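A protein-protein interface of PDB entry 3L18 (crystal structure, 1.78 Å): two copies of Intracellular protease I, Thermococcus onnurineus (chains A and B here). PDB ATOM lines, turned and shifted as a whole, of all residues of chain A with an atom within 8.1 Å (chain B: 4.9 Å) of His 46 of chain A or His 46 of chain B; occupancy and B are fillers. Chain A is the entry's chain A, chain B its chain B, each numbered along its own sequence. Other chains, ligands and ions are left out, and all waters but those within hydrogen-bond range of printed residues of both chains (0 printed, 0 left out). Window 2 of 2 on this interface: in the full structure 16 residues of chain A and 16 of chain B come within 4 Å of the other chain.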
ATOM      1  N   GLY A  12     -28.631   7.309   7.758  1.00  0.00           N
ATOM      2  CA  GLY A  12     -27.183   7.247   7.570  1.00  0.00           C
ATOM      3  C   GLY A  12     -26.399   7.779   8.757  1.00  0.00           C
ATOM      4  O   GLY A  12     -25.162   7.891   8.703  1.00  0.00           O
ATOM      5  N   PHE A  13     -27.096   8.120   9.836  1.00  0.00           N
ATOM      6  CA  PHE A  13     -26.394   8.617  11.028  1.00  0.00           C
ATOM      7  C   PHE A  13     -25.505   7.508  11.603  1.00  0.00           C
ATOM      8  O   PHE A  13     -25.766   6.302  11.395  1.00  0.00           O
ATOM      9  CB  PHE A  13     -27.386   9.149  12.073  1.00  0.00           C
ATOM     10  CG  PHE A  13     -28.318   8.099  12.652  1.00  0.00           C
ATOM     11  CD1 PHE A  13     -27.945   7.327  13.765  1.00  0.00           C
ATOM     12  CD2 PHE A  13     -29.578   7.914  12.120  1.00  0.00           C
ATOM     13  CE1 PHE A  13     -28.813   6.379  14.310  1.00  0.00           C
ATOM     14  CE2 PHE A  13     -30.457   6.964  12.659  1.00  0.00           C
ATOM     15  CZ  PHE A  13     -30.079   6.197  13.746  1.00  0.00           C
ATOM     16  N   GLU A  14     -24.455   7.912  12.301  1.00  0.00           N
ATOM     17  CA  GLU A  14     -23.623   6.957  13.034  1.00  0.00           C
ATOM     18  C   GLU A  14     -24.411   6.598  14.266  1.00  0.00           C
ATOM     19  O   GLU A  14     -24.642   7.452  15.126  1.00  0.00           O
ATOM     20  CB  GLU A  14     -22.290   7.577  13.430  1.00  0.00           C
ATOM     21  CG  GLU A  14     -21.374   6.606  14.193  1.00  0.00           C
ATOM     22  CD  GLU A  14     -20.904   5.494  13.311  1.00  0.00           C
ATOM     23  OE1 GLU A  14     -21.144   4.313  13.631  1.00  0.00           O
ATOM     24  OE2 GLU A  14     -20.314   5.809  12.258  1.00  0.00           O
ATOM     25  N   ASP A  15     -24.778   5.322  14.362  1.00  0.00           N
ATOM     26  CA  ASP A  15     -25.781   4.873  15.312  1.00  0.00           C
ATOM     27  C   ASP A  15     -25.447   5.281  16.724  1.00  0.00           C
ATOM     28  O   ASP A  15     -26.295   5.845  17.426  1.00  0.00           O
ATOM     29  CB  ASP A  15     -25.952   3.352  15.219  1.00  0.00           C
ATOM     30  CG  ASP A  15     -26.228   2.895  13.804  1.00  0.00           C
ATOM     31  OD1 ASP A  15     -25.429   3.239  12.905  1.00  0.00           O
ATOM     32  OD2 ASP A  15     -27.232   2.180  13.602  1.00  0.00           O
ATOM     33  N   LEU A  16     -24.215   4.992  17.146  1.00  0.00           N
ATOM     34  CA  LEU A  16     -23.803   5.289  18.518  1.00  0.00           C
ATOM     35  C   LEU A  16     -23.840   6.796  18.810  1.00  0.00           C
ATOM     36  O   LEU A  16     -24.211   7.211  19.905  1.00  0.00           O
ATOM     37  CB  LEU A  16     -22.392   4.736  18.796  1.00  0.00           C
ATOM     38  CG  LEU A  16     -22.182   3.225  18.935  1.00  0.00           C
ATOM     39  CD1 LEU A  16     -20.685   2.941  18.927  1.00  0.00           C
ATOM     40  CD2 LEU A  16     -22.793   2.709  20.239  1.00  0.00           C
ATOM     41  N   THR A  43     -32.804   5.585  10.004  1.00  0.00           N
ATOM     42  CA  THR A  43     -32.056   4.351  10.218  1.00  0.00           C
ATOM     43  C   THR A  43     -30.573   4.632  10.092  1.00  0.00           C
ATOM     44  O   THR A  43     -30.153   5.317   9.168  1.00  0.00           O
ATOM     45  CB  THR A  43     -32.464   3.303   9.193  1.00  0.00           C
ATOM     46  OG1 THR A  43     -33.881   3.125   9.275  1.00  0.00           O
ATOM     47  CG2 THR A  43     -31.775   1.972   9.491  1.00  0.00           C
ATOM     48  N   GLY A  44     -29.796   4.110  11.038  1.00  0.00           N
ATOM     49  CA  GLY A  44     -28.370   4.362  11.078  1.00  0.00           C
ATOM     50  C   GLY A  44     -27.581   3.511  10.118  1.00  0.00           C
ATOM     51  O   GLY A  44     -28.108   2.526   9.557  1.00  0.00           O
ATOM     52  N   LYS A  45     -26.318   3.902   9.930  1.00  0.00           N
ATOM     53  CA  LYS A  45     -25.320   3.110   9.186  1.00  0.00           C
ATOM     54  C   LYS A  45     -25.334   1.631   9.547  1.00  0.00           C
ATOM     55  O   LYS A  45     -25.146   0.780   8.669  1.00  0.00           O
ATOM     56  CB  LYS A  45     -23.916   3.669   9.421  1.00  0.00           C
ATOM     57  CG  LYS A  45     -23.594   4.910   8.564  1.00  0.00           C
ATOM     58  CD  LYS A  45     -22.363   5.676   9.056  1.00  0.00           C
ATOM     59  CE  LYS A  45     -21.059   4.936   8.763  1.00  0.00           C
ATOM     60  NZ  LYS A  45     -19.905   5.633   9.439  1.00  0.00           N
ATOM     61  N   HIS A  46     -25.538   1.332  10.835  1.00  0.00           N
ATOM     62  CA  HIS A  46     -25.477  -0.039  11.355  1.00  0.00           C
ATOM     63  C   HIS A  46     -26.844  -0.626  11.616  1.00  0.00           C
ATOM     64  O   HIS A  46     -26.956  -1.678  12.255  1.00  0.00           O
ATOM     65  CB  HIS A  46     -24.645  -0.102  12.644  1.00  0.00           C
ATOM     66  CG  HIS A  46     -23.217   0.280  12.453  1.00  0.00           C
ATOM     67  ND1 HIS A  46     -22.194  -0.647  12.426  1.00  0.00           N
ATOM     68  CD2 HIS A  46     -22.635   1.491  12.289  1.00  0.00           C
ATOM     69  CE1 HIS A  46     -21.045  -0.020  12.243  1.00  0.00           C
ATOM     70  NE2 HIS A  46     -21.287   1.278  12.149  1.00  0.00           N
ATOM     71  N   GLY A  47     -27.896   0.045  11.148  1.00  0.00           N
ATOM     72  CA  GLY A  47     -29.222  -0.567  11.159  1.00  0.00           C
ATOM     73  C   GLY A  47     -30.156  -0.250  12.305  1.00  0.00           C
ATOM     74  O   GLY A  47     -31.319  -0.660  12.283  1.00  0.00           O
ATOM     75  N   TYR A  48     -29.685   0.483  13.311  1.00  0.00           N
ATOM     76  CA  TYR A  48     -30.562   0.859  14.406  1.00  0.00           C
ATOM     77  C   TYR A  48     -31.534   1.949  13.944  1.00  0.00           C
ATOM     78  O   TYR A  48     -31.174   2.790  13.110  1.00  0.00           O
ATOM     79  CB  TYR A  48     -29.750   1.356  15.604  1.00  0.00           C
ATOM     80  CG  TYR A  48     -29.053   0.282  16.437  1.00  0.00           C
ATOM     81  CD1 TYR A  48     -27.661   0.152  16.415  1.00  0.00           C
ATOM     82  CD2 TYR A  48     -29.771  -0.556  17.288  1.00  0.00           C
ATOM     83  CE1 TYR A  48     -27.010  -0.797  17.202  1.00  0.00           C
ATOM     84  CE2 TYR A  48     -29.109  -1.522  18.092  1.00  0.00           C
ATOM     85  CZ  TYR A  48     -27.729  -1.623  18.031  1.00  0.00           C
ATOM     86  OH  TYR A  48     -27.057  -2.551  18.815  1.00  0.00           O
ATOM     87  N   SER A  49     -32.754   1.928  14.480  1.00  0.00           N
ATOM     88  CA  SER A  49     -33.789   2.925  14.112  1.00  0.00           C
ATOM     89  C   SER A  49     -34.059   3.911  15.238  1.00  0.00           C
ATOM     90  O   SER A  49     -34.005   3.552  16.414  1.00  0.00           O
ATOM     91  CB  SER A  49     -35.108   2.237  13.753  1.00  0.00           C
ATOM     92  OG  SER A  49     -35.065   1.830  12.412  1.00  0.00           O
ATOM     93  N   PRO A 153     -16.722   7.627  17.789  1.00  0.00           N
ATOM     94  CA  PRO A 153     -17.337   6.913  18.918  1.00  0.00           C
ATOM     95  C   PRO A 153     -16.431   6.504  20.094  1.00  0.00           C
ATOM     96  O   PRO A 153     -16.952   6.242  21.178  1.00  0.00           O
ATOM     97  CB  PRO A 153     -17.994   5.687  18.251  1.00  0.00           C
ATOM     98  CG  PRO A 153     -18.194   6.102  16.854  1.00  0.00           C
ATOM     99  CD  PRO A 153     -17.018   6.959  16.509  1.00  0.00           C
ATOM    100  N   GLU B  14     -25.129  -7.466  21.702  1.00  0.00           N
ATOM    101  CA  GLU B  14     -25.970  -6.373  21.234  1.00  0.00           C
ATOM    102  C   GLU B  14     -25.166  -5.096  21.400  1.00  0.00           C
ATOM    103  O   GLU B  14     -24.857  -4.704  22.513  1.00  0.00           O
ATOM    104  CB  GLU B  14     -27.242  -6.310  22.062  1.00  0.00           C
ATOM    105  CG  GLU B  14     -28.219  -5.216  21.647  1.00  0.00           C
ATOM    106  CD  GLU B  14     -28.650  -5.337  20.230  1.00  0.00           C
ATOM    107  OE1 GLU B  14     -28.528  -4.340  19.485  1.00  0.00           O
ATOM    108  OE2 GLU B  14     -29.111  -6.435  19.852  1.00  0.00           O
ATOM    109  N   ASP B  15     -24.810  -4.479  20.283  1.00  0.00           N
ATOM    110  CA  ASP B  15     -23.790  -3.428  20.270  1.00  0.00           C
ATOM    111  C   ASP B  15     -24.049  -2.356  21.307  1.00  0.00           C
ATOM    112  O   ASP B  15     -23.168  -2.027  22.088  1.00  0.00           O
ATOM    113  CB  ASP B  15     -23.668  -2.811  18.866  1.00  0.00           C
ATOM    114  CG  ASP B  15     -23.459  -3.864  17.791  1.00  0.00           C
ATOM    115  OD1 ASP B  15     -24.245  -4.816  17.765  1.00  0.00           O
ATOM    116  OD2 ASP B  15     -22.522  -3.743  16.969  1.00  0.00           O
ATOM    117  N   GLY B  44     -20.001  -6.979  17.531  1.00  0.00           N
ATOM    118  CA  GLY B  44     -21.419  -7.010  17.848  1.00  0.00           C
ATOM    119  C   GLY B  44     -22.267  -7.477  16.684  1.00  0.00           C
ATOM    120  O   GLY B  44     -21.794  -7.570  15.539  1.00  0.00           O
ATOM    121  N   LYS B  45     -23.537  -7.744  16.989  1.00  0.00           N
ATOM    122  CA  LYS B  45     -24.553  -8.067  15.988  1.00  0.00           C
ATOM    123  C   LYS B  45     -24.617  -7.044  14.866  1.00  0.00           C
ATOM    124  O   LYS B  45     -24.827  -7.408  13.713  1.00  0.00           O
ATOM    125  CB  LYS B  45     -25.917  -8.140  16.650  1.00  0.00           C
ATOM    126  CG  LYS B  45     -26.082  -9.307  17.587  1.00  0.00           C
ATOM    127  CD  LYS B  45     -27.474  -9.311  18.238  1.00  0.00           C
ATOM    128  CE  LYS B  45     -28.599  -9.328  17.180  1.00  0.00           C
ATOM    129  NZ  LYS B  45     -29.883  -8.937  17.834  1.00  0.00           N
ATOM    130  N   HIS B  46     -24.427  -5.767  15.199  1.00  0.00           N
ATOM    131  CA  HIS B  46     -24.493  -4.709  14.193  1.00  0.00           C
ATOM    132  C   HIS B  46     -23.117  -4.253  13.699  1.00  0.00           C
ATOM    133  O   HIS B  46     -23.016  -3.234  13.015  1.00  0.00           O
ATOM    134  CB  HIS B  46     -25.271  -3.496  14.721  1.00  0.00           C
ATOM    135  CG  HIS B  46     -26.690  -3.789  15.085  1.00  0.00           C
ATOM    136  ND1 HIS B  46     -27.758  -3.355  14.328  1.00  0.00           N
ATOM    137  CD2 HIS B  46     -27.221  -4.437  16.149  1.00  0.00           C
ATOM    138  CE1 HIS B  46     -28.888  -3.736  14.901  1.00  0.00           C
ATOM    139  NE2 HIS B  46     -28.591  -4.399  16.007  1.00  0.00           N
ATOM    140  N   GLY B  47     -22.066  -4.995  14.046  1.00  0.00           N
ATOM    141  CA  GLY B  47     -20.757  -4.797  13.424  1.00  0.00           C
ATOM    142  C   GLY B  47     -19.770  -3.891  14.139  1.00  0.00           C
ATOM    143  O   GLY B  47     -18.653  -3.703  13.660  1.00  0.00           O
ATOM    144  N   TYR B  48     -20.155  -3.305  15.267  1.00  0.00           N
ATOM    145  CA  TYR B  48     -19.188  -2.538  16.056  1.00  0.00           C
ATOM    146  C   TYR B  48     -18.205  -3.500  16.745  1.00  0.00           C
ATOM    147  O   TYR B  48     -18.589  -4.606  17.146  1.00  0.00           O
ATOM    148  CB  TYR B  48     -19.901  -1.655  17.092  1.00  0.00           C
ATOM    149  CG  TYR B  48     -20.596  -0.423  16.564  1.00  0.00           C
ATOM    150  CD1 TYR B  48     -21.995  -0.331  16.568  1.00  0.00           C
ATOM    151  CD2 TYR B  48     -19.868   0.681  16.111  1.00  0.00           C
ATOM    152  CE1 TYR B  48     -22.656   0.832  16.111  1.00  0.00           C
ATOM    153  CE2 TYR B  48     -20.523   1.852  15.639  1.00  0.00           C
ATOM    154  CZ  TYR B  48     -21.911   1.913  15.645  1.00  0.00           C
ATOM    155  OH  TYR B  48     -22.572   3.053  15.204  1.00  0.00           O
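The side-chain hydroxyl (OH) of Tyr 48 of chain B sits at hydrogen-bond distance from the side-chain carboxylate (OE1) of Glu 14 of chain A (2.5 Å).
The backbone NH of Asp 15 of chain A sits at hydrogen-bond distance from the side-chain hydroxyl of Tyr 48 of chain B, 3.3 Å away.
The backbone NH of Leu 16 of chain A is in hydrogen-bond range of the side-chain hydroxyl of Tyr 48 of chain B.
A ring nitrogen (ND1) of His 46 of chain A is in hydrogen-bond range of the backbone carbonyl oxygen (O) of His 46 of chain B (2.8 Å).
OH of Tyr 48 of chain A is in hydrogen-bond range of OE1 of Glu 14 of chain B (2.4 Å).
OH of Tyr 48 of chain A sits at hydrogen-bond distance from N of Asp 15 of chain B (3.3 Å).
The side-chain carboxylate (OE2) of Glu 14 of chain A is in salt-bridge range of the side-chain amino group (NZ) of Lys 45 of chain A, 2.9 Å away.
The side-chain carboxylate (OE1) of Glu 14 of chain A lies within hydrogen-bond range of a ring nitrogen (NE2) of His 46 of chain A, 3.4 Å away.
The backbone NH of Tyr 48 of chain A is in hydrogen-bond range of the side-chain carboxylate of Asp 15 of chain A (3.0 Å).
The side-chain carboxylate (OD1) of Asp 15 of chain B sits at hydrogen-bond distance from the backbone NH (N) of Lys 45 of chain B (3.1 Å).
OD1 of Asp 15 of chain B sits at hydrogen-bond distance from N of His 46 of chain B, at 2.7 Å.
The backbone NH of Gly 47 of chain B sits at hydrogen-bond distance from the side-chain carboxylate of Asp 15 of chain B.
Among the printed residues, merely in contact across the chains: Tyr 48 of chain A with His 46 of chain B (3.3 Å) and His 46 of chain A with Tyr 48 of chain B (3.3 Å).
Of the printed residues of chain B, Asp 15 of chain A touches Tyr 48 (3.3 Å).
Printed residues of chain B within 4 Å of Leu 16 of chain A: Tyr 48 (3.2 Å).
His 46 of chain A touches two residues of chain B.
Printed residues of chain A within 4 Å of Asp 15 of chain B: Tyr 48.
His 46 of chain B touches just these residues of chain A: His 46 (2.8 Å) and Tyr 48 (3.3 Å).
Hydrophobic or aromatic side chains of chain A within 4 Å of the printed part of chain B: Leu 16, His 46 and Tyr 48.
Hydrophobic or aromatic side chains of chain B within 4 Å of the printed part of chain A: His 46 and Tyr 48.
Glu 14 of chain A touches Tyr 48 of chain B, and with the chains exchanged Tyr 48 of chain A touches Glu 14 of chain B.
Asp 15 of chain A touches Tyr 48 of chain B, and with the chains exchanged Tyr 48 of chain A touches Asp 15 of chain B.
His 46 of chain B touches its own counterpart, His 46 of chain A.
His 46 of chain A touches Tyr 48 of chain B, and with the chains exchanged Tyr 48 of chain A touches His 46 of chain B.
Positions printed for both chains: 14, 15, 44, 45, 46, 47 and 48.
Of the 8 pairs that touch across the chains among the printed residues, 7 have their exchanged pair printed and touching as well.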
